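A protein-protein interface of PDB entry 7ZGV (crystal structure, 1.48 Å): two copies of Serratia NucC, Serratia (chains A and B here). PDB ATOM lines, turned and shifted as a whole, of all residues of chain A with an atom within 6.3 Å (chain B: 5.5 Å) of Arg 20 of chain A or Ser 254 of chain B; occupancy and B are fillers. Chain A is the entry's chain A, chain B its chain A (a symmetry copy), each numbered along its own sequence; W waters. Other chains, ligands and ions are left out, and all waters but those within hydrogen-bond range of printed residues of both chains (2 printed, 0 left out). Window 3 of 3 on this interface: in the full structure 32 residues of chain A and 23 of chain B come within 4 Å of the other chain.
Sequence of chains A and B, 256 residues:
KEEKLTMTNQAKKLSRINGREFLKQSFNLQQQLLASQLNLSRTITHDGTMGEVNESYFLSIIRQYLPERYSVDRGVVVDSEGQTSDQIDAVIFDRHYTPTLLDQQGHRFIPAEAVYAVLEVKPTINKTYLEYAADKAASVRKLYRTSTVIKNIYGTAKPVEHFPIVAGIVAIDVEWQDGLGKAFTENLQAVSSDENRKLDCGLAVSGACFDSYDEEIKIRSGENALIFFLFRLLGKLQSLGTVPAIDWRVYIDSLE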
ATOM      1  N   ASN A  18      -6.998 -21.717  26.391  1.00  0.00           N
ATOM      2  CA  ASN A  18      -6.693 -20.458  27.053  1.00  0.00           C
ATOM      3  C   ASN A  18      -5.897 -19.526  26.130  1.00  0.00           C
ATOM      4  O   ASN A  18      -5.464 -19.904  25.037  1.00  0.00           O
ATOM      5  CB  ASN A  18      -5.956 -20.720  28.369  1.00  0.00           C
ATOM      6  CG  ASN A  18      -4.630 -21.445  28.172  1.00  0.00           C
ATOM      7  OD1 ASN A  18      -3.662 -20.858  27.715  1.00  0.00           O
ATOM      8  ND2 ASN A  18      -4.591 -22.734  28.497  1.00  0.00           N
ATOM      9  N   GLY A  19      -5.725 -18.280  26.581  1.00  0.00           N
ATOM     10  CA  GLY A  19      -5.085 -17.272  25.752  1.00  0.00           C
ATOM     11  C   GLY A  19      -3.658 -17.621  25.351  1.00  0.00           C
ATOM     12  O   GLY A  19      -3.272 -17.427  24.204  1.00  0.00           O
ATOM     13  N   ARG A  20      -2.837 -18.098  26.302  1.00  0.00           N
ATOM     14  CA  ARG A  20      -1.456 -18.428  25.967  1.00  0.00           C
ATOM     15  C   ARG A  20      -1.417 -19.561  24.950  1.00  0.00           C
ATOM     16  O   ARG A  20      -0.652 -19.533  23.979  1.00  0.00           O
ATOM     17  CB  ARG A  20      -0.675 -18.791  27.236  1.00  0.00           C
ATOM     18  CG  ARG A  20       0.755 -19.171  26.993  1.00  0.00           C
ATOM     19  CD  ARG A  20       1.491 -19.493  28.291  1.00  0.00           C
ATOM     20  NE  ARG A  20       2.883 -19.843  28.085  1.00  0.00           N
ATOM     21  CZ  ARG A  20       3.297 -21.066  27.808  1.00  0.00           C
ATOM     22  NH1 ARG A  20       2.451 -22.077  27.719  1.00  0.00           N
ATOM     23  NH2 ARG A  20       4.592 -21.284  27.627  1.00  0.00           N
ATOM     24  N   GLU A  21      -2.203 -20.600  25.211  1.00  0.00           N
ATOM     25  CA  GLU A  21      -2.296 -21.742  24.310  1.00  0.00           C
ATOM     26  C   GLU A  21      -2.761 -21.318  22.924  1.00  0.00           C
ATOM     27  O   GLU A  21      -2.220 -21.779  21.917  1.00  0.00           O
ATOM     28  CB  GLU A  21      -3.270 -22.724  24.963  1.00  0.00           C
ATOM     29  CG  GLU A  21      -3.510 -24.065  24.345  1.00  0.00           C
ATOM     30  CD  GLU A  21      -4.483 -24.894  25.230  1.00  0.00           C
ATOM     31  OE1 GLU A  21      -5.335 -24.285  25.943  1.00  0.00           O
ATOM     32  OE2 GLU A  21      -4.397 -26.143  25.216  1.00  0.00           O
ATOM     33  N   PHE A  22      -3.759 -20.433  22.834  1.00  0.00           N
ATOM     34  CA  PHE A  22      -4.227 -20.006  21.525  1.00  0.00           C
ATOM     35  C   PHE A  22      -3.170 -19.193  20.795  1.00  0.00           C
ATOM     36  O   PHE A  22      -3.008 -19.326  19.582  1.00  0.00           O
ATOM     37  CB  PHE A  22      -5.503 -19.175  21.659  1.00  0.00           C
ATOM     38  CG  PHE A  22      -6.124 -18.845  20.331  1.00  0.00           C
ATOM     39  CD1 PHE A  22      -6.735 -19.837  19.582  1.00  0.00           C
ATOM     40  CD2 PHE A  22      -6.053 -17.570  19.812  1.00  0.00           C
ATOM     41  CE1 PHE A  22      -7.263 -19.577  18.354  1.00  0.00           C
ATOM     42  CE2 PHE A  22      -6.598 -17.295  18.585  1.00  0.00           C
ATOM     43  CZ  PHE A  22      -7.208 -18.275  17.857  1.00  0.00           C
ATOM     44  N   LEU A  23      -2.444 -18.333  21.508  1.00  0.00           N
ATOM     45  CA  LEU A  23      -1.355 -17.601  20.873  1.00  0.00           C
ATOM     46  C   LEU A  23      -0.319 -18.547  20.290  1.00  0.00           C
ATOM     47  O   LEU A  23       0.077 -18.414  19.117  1.00  0.00           O
ATOM     48  CB  LEU A  23      -0.731 -16.650  21.898  1.00  0.00           C
ATOM     49  CG  LEU A  23       0.437 -15.816  21.378  1.00  0.00           C
ATOM     50  CD1 LEU A  23       0.057 -14.862  20.285  1.00  0.00           C
ATOM     51  CD2 LEU A  23       1.121 -15.072  22.506  1.00  0.00           C
ATOM     52  N   LYS A  24       0.127 -19.528  21.076  1.00  0.00           N
ATOM     53  CA  LYS A  24       1.107 -20.484  20.573  1.00  0.00           C
ATOM     54  C   LYS A  24       0.591 -21.222  19.349  1.00  0.00           C
ATOM     55  O   LYS A  24       1.341 -21.453  18.389  1.00  0.00           O
ATOM     56  CB  LYS A  24       1.441 -21.492  21.670  1.00  0.00           C
ATOM     57  CG  LYS A  24       2.268 -20.939  22.804  1.00  0.00           C
ATOM     58  CD  LYS A  24       2.505 -21.985  23.884  1.00  0.00           C
ATOM     59  CE  LYS A  24       3.083 -23.267  23.320  1.00  0.00           C
ATOM     60  NZ  LYS A  24       3.735 -24.079  24.341  1.00  0.00           N
ATOM     61  N   GLN A  25      -0.648 -21.710  19.406  1.00  0.00           N
ATOM     62  CA  GLN A  25      -1.206 -22.472  18.281  1.00  0.00           C
ATOM     63  C   GLN A  25      -1.390 -21.626  17.040  1.00  0.00           C
ATOM     64  O   GLN A  25      -1.155 -22.100  15.902  1.00  0.00           O
ATOM     65  CB  GLN A  25      -2.530 -23.110  18.715  1.00  0.00           C
ATOM     66  CG  GLN A  25      -2.282 -24.274  19.657  1.00  0.00           C
ATOM     67  CD  GLN A  25      -3.535 -24.937  20.198  1.00  0.00           C
ATOM     68  OE1 GLN A  25      -4.651 -24.732  19.723  1.00  0.00           O
ATOM     69  NE2 GLN A  25      -3.351 -25.720  21.232  1.00  0.00           N
ATOM     70  N   VAL B  78      -6.374  -9.964  24.274  1.00  0.00           N
ATOM     71  CA  VAL B  78      -5.455 -10.797  25.040  1.00  0.00           C
ATOM     72  C   VAL B  78      -4.301  -9.922  25.513  1.00  0.00           C
ATOM     73  O   VAL B  78      -3.974  -8.916  24.885  1.00  0.00           O
ATOM     74  CB  VAL B  78      -4.927 -11.954  24.162  1.00  0.00           C
ATOM     75  CG1 VAL B  78      -4.075 -11.426  23.004  1.00  0.00           C
ATOM     76  CG2 VAL B  78      -4.125 -12.953  25.006  1.00  0.00           C
ATOM     77  N   GLY B  82      -1.178 -13.781  29.119  1.00  0.00           N
ATOM     78  CA  GLY B  82      -2.040 -14.874  28.691  1.00  0.00           C
ATOM     79  C   GLY B  82      -3.500 -14.715  29.053  1.00  0.00           C
ATOM     80  O   GLY B  82      -4.291 -15.639  28.829  1.00  0.00           O
ATOM     81  N   VAL B 250       7.386  -9.204  25.778  1.00  0.00           N
ATOM     82  CA  VAL B 250       6.538  -9.840  26.785  1.00  0.00           C
ATOM     83  C   VAL B 250       5.562 -10.838  26.192  1.00  0.00           C
ATOM     84  O   VAL B 250       4.977 -11.643  26.943  1.00  0.00           O
ATOM     85  CB  VAL B 250       5.738  -8.813  27.612  1.00  0.00           C
ATOM     86  CG1 VAL B 250       6.680  -7.968  28.436  1.00  0.00           C
ATOM     87  CG2 VAL B 250       4.874  -7.954  26.716  1.00  0.00           C
ATOM     88  N   ILE B 252       6.583 -13.160  24.129  1.00  0.00           N
ATOM     89  CA  ILE B 252       7.366 -14.365  23.878  1.00  0.00           C
ATOM     90  C   ILE B 252       8.192 -14.809  25.079  1.00  0.00           C
ATOM     91  O   ILE B 252       8.928 -15.789  24.981  1.00  0.00           O
ATOM     92  CB  ILE B 252       8.249 -14.229  22.614  1.00  0.00           C
ATOM     93  CG1 ILE B 252       9.150 -12.997  22.753  1.00  0.00           C
ATOM     94  CG2 ILE B 252       7.376 -14.149  21.350  1.00  0.00           C
ATOM     95  CD1 ILE B 252      10.265 -12.925  21.675  1.00  0.00           C
ATOM     96  N   ASP B 253       8.080 -14.131  26.221  1.00  0.00           N
ATOM     97  CA  ASP B 253       8.977 -14.409  27.336  1.00  0.00           C
ATOM     98  C   ASP B 253       8.681 -15.716  28.068  1.00  0.00           C
ATOM     99  O   ASP B 253       9.578 -16.236  28.734  1.00  0.00           O
ATOM    100  CB  ASP B 253       9.037 -13.226  28.308  1.00  0.00           C
ATOM    101  CG  ASP B 253       7.670 -12.855  28.889  1.00  0.00           C
ATOM    102  OD1 ASP B 253       6.646 -13.530  28.589  1.00  0.00           O
ATOM    103  OD2 ASP B 253       7.648 -11.870  29.666  1.00  0.00           O
ATOM    104  N   SER B 254       7.480 -16.281  27.941  1.00  0.00           N
ATOM    105  CA  SER B 254       7.182 -17.548  28.586  1.00  0.00           C
ATOM    106  C   SER B 254       7.347 -18.741  27.657  1.00  0.00           C
ATOM    107  O   SER B 254       7.078 -19.871  28.081  1.00  0.00           O
ATOM    108  CB  SER B 254       5.752 -17.550  29.129  1.00  0.00           C
ATOM    109  OG  SER B 254       4.841 -17.713  28.062  1.00  0.00           O
ATOM    110  N   LEU B 255       7.796 -18.529  26.417  1.00  0.00           N
ATOM    111  CA  LEU B 255       7.903 -19.603  25.436  1.00  0.00           C
ATOM    112  C   LEU B 255       9.300 -20.210  25.404  1.00  0.00           C
ATOM    113  O   LEU B 255      10.304 -19.525  25.612  1.00  0.00           O
ATOM    114  CB  LEU B 255       7.546 -19.054  24.049  1.00  0.00           C
ATOM    115  CG  LEU B 255       6.179 -18.388  23.977  1.00  0.00           C
ATOM    116  CD1 LEU B 255       5.956 -17.782  22.589  1.00  0.00           C
ATOM    117  CD2 LEU B 255       5.072 -19.384  24.343  1.00  0.00           C
ATOM    118  N   GLU B 256       9.353 -21.510  25.164  1.00  0.00           N
ATOM    119  CA  GLU B 256      10.636 -22.180  25.037  1.00  0.00           C
ATOM    120  C   GLU B 256      11.023 -22.359  23.569  1.00  0.00           C
ATOM    121  O   GLU B 256      10.180 -22.346  22.670  1.00  0.00           O
ATOM    122  CB  GLU B 256      10.633 -23.527  25.767  1.00  0.00           C
ATOM    123  CG  GLU B 256      11.982 -24.261  25.680  1.00  0.00           C
ATOM    124  CD  GLU B 256      12.328 -25.056  26.939  1.00  0.00           C
ATOM    125  OE1 GLU B 256      11.609 -24.917  27.954  1.00  0.00           O
ATOM    126  OE2 GLU B 256      13.320 -25.825  26.913  1.00  0.00           O
ATOM    127  OXT GLU B 256      12.198 -22.503  23.241  1.00  0.00           O
HETATM  128  O   HOH W   1       6.473 -23.066  25.095  1.00  0.00           O
HETATM  129  O   HOH W   2      -3.584 -18.233  29.314  1.00  0.00           O
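The guanidinium group (NE) of Arg 20 of chain A sits at hydrogen-bond distance from the side-chain hydroxyl (OG) of Ser 254 of chain B, 2.9 Å away.
The side-chain amide oxygen (OD1) of Asn 18 of chain A sits at hydrogen-bond distance from the backbone NH (N) of Arg 20 of chain A (3.2 Å).
CA of Gly 19 of chain A touches O of Gly 82 of chain B, 3.6 Å away. O of Gly 82 of chain B touches N of Arg 20 of chain A, at 3.8 Å. Leu 255 of chain B touches Arg 20 of chain A (CD2 to NH2, 3.8 Å). Lys 24 of chain A touches Leu 255 of chain B.
Arg 20 of chain A touches just these residues of chain B: Gly 82 (3.8 Å), Ser 254 (2.9 Å) and Leu 255 (3.8 Å). Of chain A, only Arg 20 comes within 4 Å of Ser 254 of chain B. Of the printed residues of chain A, Leu 255 of chain B touches Arg 20 and Lys 24. Of the printed residues of chain B, Gly 19 of chain A touches Gly 82 (3.6 Å). Of the printed residues of chain B, Lys 24 of chain A touches Leu 255 (3.6 Å). The nearest residue of chain B that does not touch Arg 20 of chain A is Glu 256 of chain B (5.4 Å).
Printed residues of chain B that touch a printed residue of chain A: Gly 82, Ser 254 and Leu 255. Hydrophobic or aromatic side chains of chain B that line the printed part of chain A: Leu 255. Of the 8 printed residues of chain A, 3 touch a printed residue of chain B. Printed residues of chain A that touch a printed residue of chain B: Gly 19, Arg 20 and Lys 24. Among the printed residues, 5 pairs touch across the chains. Among the printed residues, no Asp or Glu carboxylate lies within 4 Å of a Lys or Arg side-chain nitrogen of the other chain.
No position is printed for both chains. Of the 5 pairs that touch across the chains among the printed residues, none has its exchanged pair printed and touching as well.
Water W2 lies within hydrogen-bond range of O of Gly 82 of chain B (2.7 Å), OD1 of Asn 18 of chain A (3.1 Å), N of Arg 20 of chain A (3.1 Å) and N of Gly 19 of chain A (3.5 Å). Water W1 bridges the side-chain amino group of Lys 24 of chain A and the backbone NH of Glu 256 of chain B.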
